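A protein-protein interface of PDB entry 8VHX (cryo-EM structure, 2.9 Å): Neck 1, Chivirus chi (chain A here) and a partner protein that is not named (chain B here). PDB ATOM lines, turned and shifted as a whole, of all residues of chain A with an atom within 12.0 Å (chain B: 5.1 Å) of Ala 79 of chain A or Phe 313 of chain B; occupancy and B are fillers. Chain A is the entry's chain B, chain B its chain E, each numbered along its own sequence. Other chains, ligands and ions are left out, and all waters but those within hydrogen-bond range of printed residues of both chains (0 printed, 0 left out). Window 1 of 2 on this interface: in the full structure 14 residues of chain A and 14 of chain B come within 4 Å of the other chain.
The backbone NH (N) of Met 318 of chain B is in hydrogen-bond range of the backbone carbonyl oxygen (O) of Phe 313 of chain B, 2.7 Å away. The side-chain amino group of Lys 342 of chain B lies within salt-bridge range of the side-chain carboxylate of Asp 310 of chain B, at 3.99 Å.
The backbone carbonyl oxygen of Ile 344 of chain B is in hydrogen-bond range of the backbone NH of Leu 82 of chain A (2.8 Å). O of Gly 80 of chain A lies within hydrogen-bond range of N of Ile 344 of chain B. N of Gly 80 of chain A sits at hydrogen-bond distance from O of Lys 342 of chain B (3.4 Å).
Among the printed residues, pairs that only touch across the chains: Phe 81 of chain A with Ile 344 of chain B, Ala 79 of chain A with Ile 344 of chain B, Ala 79 of chain A with Phe 313 of chain B, Ser 77 of chain A with Phe 313 of chain B, Val 56 of chain A with Val 311 of chain B, Ser 77 of chain A with Lys 342 of chain B and Asn 60 of chain A with Asp 310 of chain B.
Printed residues of chain B that touch a printed residue of chain A: Asp 310, Val 311, Phe 313, Lys 342 and Ile 344. Along chain B the printed residues that touch a printed residue of chain A span positions 310 to 344. Among the printed residues, 10 pairs touch across the chains.
Of the printed residues of chain B, Val 56 of chain A touches Val 311 (3.6 Å). Printed residues of chain B within 4 Å of Asn 60 of chain A: Asp 310. Pro 78 of chain A touches none of the printed residues of chain B. Of the printed residues of chain B, Ala 79 of chain A touches Phe 313 and Ile 344. Printed residues of chain B within 4 Å of Phe 81 of chain A: Ile 344 (3.1 Å). No residue of chain A comes within 4 Å of Ile 303 of chain B. Val 311 of chain B touches just one residue of chain A: Val 56 (3.6 Å). Val 312 of chain B touches none of the printed residues of chain A. Of chain A, only Ser 77 (3.5 Å) and Ala 79 (3.5 Å) come within 4 Å of Phe 313 of chain B. No residue of chain A comes within 4 Å of Asn 314 of chain B. No residue of chain A comes within 4 Å of Gln 315 of chain B. No residue of chain A comes within 4 Å of Met 316 of chain B. No residue of chain A comes within 4 Å of Gly 317 of chain B. No residue of chain A comes within 4 Å of Met 318 of chain B. Lys 342 of chain B touches just these residues of chain A: Ser 77 (3.6 Å) and Gly 80 (3.4 Å). Ile 344 of chain B touches just these residues of chain A: Ala 79 (3.4 Å), Gly 80 (2.6 Å), Phe 81 (3.1 Å) and Leu 82 (2.8 Å). The nearest residue of chain B that does not touch Ala 79 of chain A is Lys 342 of chain B (4.02 Å).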
ATOM      1  N   VAL A  56      30.844 -10.341   0.986  1.00  0.00           N
ATOM      2  CA  VAL A  56      30.803 -11.772   0.725  1.00  0.00           C
ATOM      3  C   VAL A  56      30.485 -12.046  -0.738  1.00  0.00           C
ATOM      4  O   VAL A  56      31.075 -12.939  -1.352  1.00  0.00           O
ATOM      5  CB  VAL A  56      29.792 -12.450   1.658  1.00  0.00           C
ATOM      6  CG1 VAL A  56      29.719 -13.894   1.372  1.00  0.00           C
ATOM      7  CG2 VAL A  56      30.177 -12.254   3.067  1.00  0.00           C
ATOM      8  N   ARG A  57      29.554 -11.292  -1.322  1.00  0.00           N
ATOM      9  CA  ARG A  57      29.296 -11.433  -2.752  1.00  0.00           C
ATOM     10  C   ARG A  57      30.572 -11.237  -3.542  1.00  0.00           C
ATOM     11  O   ARG A  57      30.911 -12.037  -4.421  1.00  0.00           O
ATOM     12  CB  ARG A  57      28.276 -10.412  -3.241  1.00  0.00           C
ATOM     13  CG  ARG A  57      26.924 -10.407  -2.610  1.00  0.00           C
ATOM     14  CD  ARG A  57      25.939  -9.868  -3.625  1.00  0.00           C
ATOM     15  NE  ARG A  57      25.559 -10.891  -4.584  1.00  0.00           N
ATOM     16  CZ  ARG A  57      24.446 -11.605  -4.512  1.00  0.00           C
ATOM     17  NH1 ARG A  57      24.195 -12.520  -5.423  1.00  0.00           N
ATOM     18  NH2 ARG A  57      23.571 -11.397  -3.547  1.00  0.00           N
ATOM     19  N   ASN A  60      33.166 -14.024  -3.040  1.00  0.00           N
ATOM     20  CA  ASN A  60      32.770 -15.259  -3.698  1.00  0.00           C
ATOM     21  C   ASN A  60      32.915 -15.144  -5.204  1.00  0.00           C
ATOM     22  O   ASN A  60      33.263 -16.121  -5.875  1.00  0.00           O
ATOM     23  CB  ASN A  60      31.341 -15.616  -3.324  1.00  0.00           C
ATOM     24  CG  ASN A  60      30.936 -16.964  -3.831  1.00  0.00           C
ATOM     25  OD1 ASN A  60      31.460 -17.986  -3.398  1.00  0.00           O
ATOM     26  ND2 ASN A  60      29.995 -16.981  -4.757  1.00  0.00           N
ATOM     27  N   ALA A  70      28.754 -15.075 -10.845  1.00  0.00           N
ATOM     28  CA  ALA A  70      28.664 -15.474  -9.448  1.00  0.00           C
ATOM     29  C   ALA A  70      28.263 -14.320  -8.546  1.00  0.00           C
ATOM     30  O   ALA A  70      27.708 -14.542  -7.465  1.00  0.00           O
ATOM     31  CB  ALA A  70      29.994 -16.050  -8.981  1.00  0.00           C
ATOM     32  N   MET A  72      25.925 -11.982  -9.119  1.00  0.00           N
ATOM     33  CA  MET A  72      24.474 -11.889  -9.083  1.00  0.00           C
ATOM     34  C   MET A  72      23.841 -13.195  -8.622  1.00  0.00           C
ATOM     35  O   MET A  72      22.789 -13.185  -7.975  1.00  0.00           O
ATOM     36  CB  MET A  72      23.957 -11.502 -10.459  1.00  0.00           C
ATOM     37  CG  MET A  72      22.808 -10.521 -10.430  1.00  0.00           C
ATOM     38  SD  MET A  72      23.357  -8.839 -10.138  1.00  0.00           S
ATOM     39  CE  MET A  72      24.307  -8.550 -11.616  1.00  0.00           C
ATOM     40  N   GLY A  73      24.463 -14.325  -8.947  1.00  0.00           N
ATOM     41  CA  GLY A  73      23.961 -15.622  -8.541  1.00  0.00           C
ATOM     42  C   GLY A  73      22.720 -16.092  -9.257  1.00  0.00           C
ATOM     43  O   GLY A  73      22.123 -17.083  -8.837  1.00  0.00           O
ATOM     44  N   LEU A  74      22.320 -15.424 -10.327  1.00  0.00           N
ATOM     45  CA  LEU A  74      21.083 -15.722 -11.034  1.00  0.00           C
ATOM     46  C   LEU A  74      21.047 -17.119 -11.637  1.00  0.00           C
ATOM     47  O   LEU A  74      19.957 -17.666 -11.844  1.00  0.00           O
ATOM     48  CB  LEU A  74      20.832 -14.689 -12.122  1.00  0.00           C
ATOM     49  CG  LEU A  74      20.500 -13.304 -11.570  1.00  0.00           C
ATOM     50  CD1 LEU A  74      20.068 -12.367 -12.690  1.00  0.00           C
ATOM     51  CD2 LEU A  74      19.437 -13.398 -10.485  1.00  0.00           C
ATOM     52  N   PRO A  75      22.171 -17.739 -11.923  1.00  0.00           N
ATOM     53  CA  PRO A  75      22.119 -19.168 -12.251  1.00  0.00           C
ATOM     54  C   PRO A  75      21.712 -19.955 -11.016  1.00  0.00           C
ATOM     55  O   PRO A  75      22.412 -20.861 -10.556  1.00  0.00           O
ATOM     56  CB  PRO A  75      23.551 -19.482 -12.705  1.00  0.00           C
ATOM     57  CG  PRO A  75      24.083 -18.171 -13.165  1.00  0.00           C
ATOM     58  CD  PRO A  75      23.481 -17.157 -12.244  1.00  0.00           C
ATOM     59  N   SER A  76      20.555 -19.582 -10.477  1.00  0.00           N
ATOM     60  CA  SER A  76      20.121 -19.983  -9.155  1.00  0.00           C
ATOM     61  C   SER A  76      19.250 -21.224  -9.219  1.00  0.00           C
ATOM     62  O   SER A  76      18.651 -21.554 -10.246  1.00  0.00           O
ATOM     63  CB  SER A  76      19.349 -18.858  -8.484  1.00  0.00           C
ATOM     64  OG  SER A  76      18.191 -18.524  -9.220  1.00  0.00           O
ATOM     65  N   SER A  77      19.178 -21.906  -8.090  1.00  0.00           N
ATOM     66  CA  SER A  77      18.349 -23.088  -7.946  1.00  0.00           C
ATOM     67  C   SER A  77      18.383 -23.511  -6.491  1.00  0.00           C
ATOM     68  O   SER A  77      19.340 -23.207  -5.780  1.00  0.00           O
ATOM     69  CB  SER A  77      18.828 -24.229  -8.853  1.00  0.00           C
ATOM     70  OG  SER A  77      18.314 -24.075 -10.160  1.00  0.00           O
ATOM     71  N   PRO A  78      17.352 -24.201  -6.036  1.00  0.00           N
ATOM     72  CA  PRO A  78      17.291 -24.592  -4.637  1.00  0.00           C
ATOM     73  C   PRO A  78      18.201 -25.764  -4.343  1.00  0.00           C
ATOM     74  O   PRO A  78      18.476 -26.605  -5.199  1.00  0.00           O
ATOM     75  CB  PRO A  78      15.824 -24.967  -4.456  1.00  0.00           C
ATOM     76  CG  PRO A  78      15.426 -25.435  -5.717  1.00  0.00           C
ATOM     77  CD  PRO A  78      16.155 -24.635  -6.747  1.00  0.00           C
ATOM     78  N   ALA A  79      18.675 -25.805  -3.108  1.00  0.00           N
ATOM     79  CA  ALA A  79      19.586 -26.856  -2.700  1.00  0.00           C
ATOM     80  C   ALA A  79      18.834 -28.155  -2.498  1.00  0.00           C
ATOM     81  O   ALA A  79      17.835 -28.204  -1.780  1.00  0.00           O
ATOM     82  CB  ALA A  79      20.296 -26.464  -1.417  1.00  0.00           C
ATOM     83  N   GLY A  80      19.327 -29.210  -3.133  1.00  0.00           N
ATOM     84  CA  GLY A  80      18.805 -30.537  -2.935  1.00  0.00           C
ATOM     85  C   GLY A  80      19.644 -31.297  -1.933  1.00  0.00           C
ATOM     86  O   GLY A  80      20.652 -30.818  -1.425  1.00  0.00           O
ATOM     87  N   PHE A  81      19.212 -32.516  -1.661  1.00  0.00           N
ATOM     88  CA  PHE A  81      19.804 -33.308  -0.607  1.00  0.00           C
ATOM     89  C   PHE A  81      20.095 -34.712  -1.095  1.00  0.00           C
ATOM     90  O   PHE A  81      19.346 -35.283  -1.890  1.00  0.00           O
ATOM     91  CB  PHE A  81      18.895 -33.338   0.598  1.00  0.00           C
ATOM     92  CG  PHE A  81      18.687 -32.006   1.198  1.00  0.00           C
ATOM     93  CD1 PHE A  81      19.631 -31.459   2.023  1.00  0.00           C
ATOM     94  CD2 PHE A  81      17.575 -31.274   0.901  1.00  0.00           C
ATOM     95  CE1 PHE A  81      19.453 -30.236   2.550  1.00  0.00           C
ATOM     96  CE2 PHE A  81      17.407 -30.049   1.431  1.00  0.00           C
ATOM     97  CZ  PHE A  81      18.343 -29.531   2.251  1.00  0.00           C
ATOM     98  N   LEU A  82      21.194 -35.256  -0.599  1.00  0.00           N
ATOM     99  CA  LEU A  82      21.583 -36.631  -0.825  1.00  0.00           C
ATOM    100  C   LEU A  82      21.612 -37.337   0.515  1.00  0.00           C
ATOM    101  O   LEU A  82      22.058 -36.767   1.512  1.00  0.00           O
ATOM    102  CB  LEU A  82      22.938 -36.723  -1.491  1.00  0.00           C
ATOM    103  CG  LEU A  82      23.015 -36.206  -2.914  1.00  0.00           C
ATOM    104  CD1 LEU A  82      24.442 -36.128  -3.334  1.00  0.00           C
ATOM    105  CD2 LEU A  82      22.264 -37.108  -3.826  1.00  0.00           C
ATOM    106  N   PHE A  83      21.141 -38.574   0.534  1.00  0.00           N
ATOM    107  CA  PHE A  83      20.920 -39.243   1.790  1.00  0.00           C
ATOM    108  C   PHE A  83      21.725 -40.531   1.864  1.00  0.00           C
ATOM    109  O   PHE A  83      21.852 -41.241   0.861  1.00  0.00           O
ATOM    110  CB  PHE A  83      19.437 -39.560   1.981  1.00  0.00           C
ATOM    111  CG  PHE A  83      18.551 -38.373   1.856  1.00  0.00           C
ATOM    112  CD1 PHE A  83      18.238 -37.608   2.948  1.00  0.00           C
ATOM    113  CD2 PHE A  83      18.049 -38.009   0.638  1.00  0.00           C
ATOM    114  CE1 PHE A  83      17.438 -36.521   2.817  1.00  0.00           C
ATOM    115  CE2 PHE A  83      17.254 -36.920   0.518  1.00  0.00           C
ATOM    116  CZ  PHE A  83      16.951 -36.179   1.606  1.00  0.00           C
ATOM    117  N   ILE B 303      15.601 -20.055   3.068  1.00  0.00           N
ATOM    118  CA  ILE B 303      16.494 -19.016   3.536  1.00  0.00           C
ATOM    119  C   ILE B 303      16.079 -17.707   2.898  1.00  0.00           C
ATOM    120  O   ILE B 303      15.804 -17.652   1.695  1.00  0.00           O
ATOM    121  CB  ILE B 303      17.960 -19.330   3.213  1.00  0.00           C
ATOM    122  CG1 ILE B 303      18.412 -20.591   3.913  1.00  0.00           C
ATOM    123  CG2 ILE B 303      18.828 -18.209   3.645  1.00  0.00           C
ATOM    124  CD1 ILE B 303      18.376 -21.747   3.059  1.00  0.00           C
ATOM    125  N   SER B 309      23.634 -17.576  -3.317  1.00  0.00           N
ATOM    126  CA  SER B 309      23.204 -18.936  -3.035  1.00  0.00           C
ATOM    127  C   SER B 309      24.381 -19.846  -2.720  1.00  0.00           C
ATOM    128  O   SER B 309      24.260 -20.778  -1.919  1.00  0.00           O
ATOM    129  CB  SER B 309      22.425 -19.466  -4.225  1.00  0.00           C
ATOM    130  OG  SER B 309      23.180 -19.321  -5.414  1.00  0.00           O
ATOM    131  N   ASP B 310      25.522 -19.607  -3.355  1.00  0.00           N
ATOM    132  CA  ASP B 310      26.662 -20.493  -3.180  1.00  0.00           C
ATOM    133  C   ASP B 310      27.218 -20.418  -1.768  1.00  0.00           C
ATOM    134  O   ASP B 310      27.710 -21.419  -1.239  1.00  0.00           O
ATOM    135  CB  ASP B 310      27.741 -20.137  -4.194  1.00  0.00           C
ATOM    136  CG  ASP B 310      27.271 -20.310  -5.624  1.00  0.00           C
ATOM    137  OD1 ASP B 310      27.140 -21.467  -6.075  1.00  0.00           O
ATOM    138  OD2 ASP B 310      27.024 -19.287  -6.298  1.00  0.00           O
ATOM    139  N   VAL B 311      27.161 -19.237  -1.159  1.00  0.00           N
ATOM    140  CA  VAL B 311      27.589 -19.071   0.225  1.00  0.00           C
ATOM    141  C   VAL B 311      26.585 -19.707   1.170  1.00  0.00           C
ATOM    142  O   VAL B 311      26.947 -20.459   2.081  1.00  0.00           O
ATOM    143  CB  VAL B 311      27.761 -17.579   0.538  1.00  0.00           C
ATOM    144  CG1 VAL B 311      27.948 -17.380   1.988  1.00  0.00           C
ATOM    145  CG2 VAL B 311      28.899 -17.014  -0.218  1.00  0.00           C
ATOM    146  N   VAL B 312      25.307 -19.400   0.970  1.00  0.00           N
ATOM    147  CA  VAL B 312      24.265 -19.842   1.885  1.00  0.00           C
ATOM    148  C   VAL B 312      24.240 -21.357   1.978  1.00  0.00           C
ATOM    149  O   VAL B 312      24.173 -21.929   3.069  1.00  0.00           O
ATOM    150  CB  VAL B 312      22.910 -19.283   1.439  1.00  0.00           C
ATOM    151  CG1 VAL B 312      21.812 -20.012   2.100  1.00  0.00           C
ATOM    152  CG2 VAL B 312      22.837 -17.849   1.766  1.00  0.00           C
ATOM    153  N   PHE B 313      24.273 -22.029   0.836  1.00  0.00           N
ATOM    154  CA  PHE B 313      24.217 -23.480   0.847  1.00  0.00           C
ATOM    155  C   PHE B 313      25.506 -24.087   1.363  1.00  0.00           C
ATOM    156  O   PHE B 313      25.490 -25.182   1.933  1.00  0.00           O
ATOM    157  CB  PHE B 313      23.923 -23.992  -0.544  1.00  0.00           C
ATOM    158  CG  PHE B 313      22.642 -23.489  -1.111  1.00  0.00           C
ATOM    159  CD1 PHE B 313      21.524 -23.356  -0.324  1.00  0.00           C
ATOM    160  CD2 PHE B 313      22.550 -23.150  -2.439  1.00  0.00           C
ATOM    161  CE1 PHE B 313      20.364 -22.902  -0.848  1.00  0.00           C
ATOM    162  CE2 PHE B 313      21.385 -22.695  -2.954  1.00  0.00           C
ATOM    163  CZ  PHE B 313      20.295 -22.571  -2.158  1.00  0.00           C
ATOM    164  N   ASN B 314      26.631 -23.411   1.155  1.00  0.00           N
ATOM    165  CA  ASN B 314      27.881 -23.865   1.743  1.00  0.00           C
ATOM    166  C   ASN B 314      27.811 -23.816   3.260  1.00  0.00           C
ATOM    167  O   ASN B 314      28.372 -24.678   3.944  1.00  0.00           O
ATOM    168  CB  ASN B 314      29.027 -23.015   1.223  1.00  0.00           C
ATOM    169  CG  ASN B 314      30.375 -23.575   1.579  1.00  0.00           C
ATOM    170  OD1 ASN B 314      30.541 -24.785   1.719  1.00  0.00           O
ATOM    171  ND2 ASN B 314      31.360 -22.698   1.708  1.00  0.00           N
ATOM    172  N   GLN B 315      27.122 -22.813   3.802  1.00  0.00           N
ATOM    173  CA  GLN B 315      26.889 -22.755   5.239  1.00  0.00           C
ATOM    174  C   GLN B 315      26.046 -23.920   5.713  1.00  0.00           C
ATOM    175  O   GLN B 315      26.207 -24.386   6.844  1.00  0.00           O
ATOM    176  CB  GLN B 315      26.192 -21.456   5.603  1.00  0.00           C
ATOM    177  CG  GLN B 315      27.017 -20.230   5.451  1.00  0.00           C
ATOM    178  CD  GLN B 315      26.207 -18.982   5.589  1.00  0.00           C
ATOM    179  OE1 GLN B 315      24.985 -19.008   5.536  1.00  0.00           O
ATOM    180  NE2 GLN B 315      26.881 -17.873   5.756  1.00  0.00           N
ATOM    181  N   MET B 316      25.133 -24.387   4.876  1.00  0.00           N
ATOM    182  CA  MET B 316      24.200 -25.431   5.253  1.00  0.00           C
ATOM    183  C   MET B 316      24.726 -26.832   4.980  1.00  0.00           C
ATOM    184  O   MET B 316      24.055 -27.804   5.338  1.00  0.00           O
ATOM    185  CB  MET B 316      22.882 -25.220   4.522  1.00  0.00           C
ATOM    186  CG  MET B 316      22.193 -23.916   4.852  1.00  0.00           C
ATOM    187  SD  MET B 316      21.690 -23.774   6.557  1.00  0.00           S
ATOM    188  CE  MET B 316      20.283 -24.846   6.479  1.00  0.00           C
ATOM    189  N   GLY B 317      25.890 -26.958   4.357  1.00  0.00           N
ATOM    190  CA  GLY B 317      26.511 -28.241   4.122  1.00  0.00           C
ATOM    191  C   GLY B 317      26.759 -28.598   2.677  1.00  0.00           C
ATOM    192  O   GLY B 317      27.059 -29.760   2.394  1.00  0.00           O
ATOM    193  N   MET B 318      26.653 -27.647   1.759  1.00  0.00           N
ATOM    194  CA  MET B 318      26.870 -27.943   0.351  1.00  0.00           C
ATOM    195  C   MET B 318      28.357 -28.102   0.084  1.00  0.00           C
ATOM    196  O   MET B 318      29.159 -27.234   0.438  1.00  0.00           O
ATOM    197  CB  MET B 318      26.279 -26.836  -0.521  1.00  0.00           C
ATOM    198  CG  MET B 318      25.977 -27.250  -1.946  1.00  0.00           C
ATOM    199  SD  MET B 318      25.052 -26.032  -2.893  1.00  0.00           S
ATOM    200  CE  MET B 318      26.357 -24.966  -3.493  1.00  0.00           C
ATOM    201  N   LYS B 342      25.169 -29.242  -6.706  1.00  0.00           N
ATOM    202  CA  LYS B 342      24.357 -28.422  -5.819  1.00  0.00           C
ATOM    203  C   LYS B 342      23.440 -29.294  -4.977  1.00  0.00           C
ATOM    204  O   LYS B 342      22.258 -28.993  -4.815  1.00  0.00           O
ATOM    205  CB  LYS B 342      23.541 -27.413  -6.623  1.00  0.00           C
ATOM    206  CG  LYS B 342      22.853 -26.336  -5.785  1.00  0.00           C
ATOM    207  CD  LYS B 342      22.191 -25.250  -6.628  1.00  0.00           C
ATOM    208  CE  LYS B 342      23.185 -24.369  -7.362  1.00  0.00           C
ATOM    209  NZ  LYS B 342      23.561 -23.152  -6.586  1.00  0.00           N
ATOM    210  N   ILE B 344      23.187 -31.144  -1.186  1.00  0.00           N
ATOM    211  CA  ILE B 344      23.702 -31.165   0.176  1.00  0.00           C
ATOM    212  C   ILE B 344      23.672 -32.591   0.701  1.00  0.00           C
ATOM    213  O   ILE B 344      22.619 -33.230   0.738  1.00  0.00           O
ATOM    214  CB  ILE B 344      22.888 -30.234   1.079  1.00  0.00           C
ATOM    215  CG1 ILE B 344      23.109 -28.780   0.702  1.00  0.00           C
ATOM    216  CG2 ILE B 344      23.242 -30.452   2.493  1.00  0.00           C
ATOM    217  CD1 ILE B 344      22.040 -27.878   1.190  1.00  0.00           C
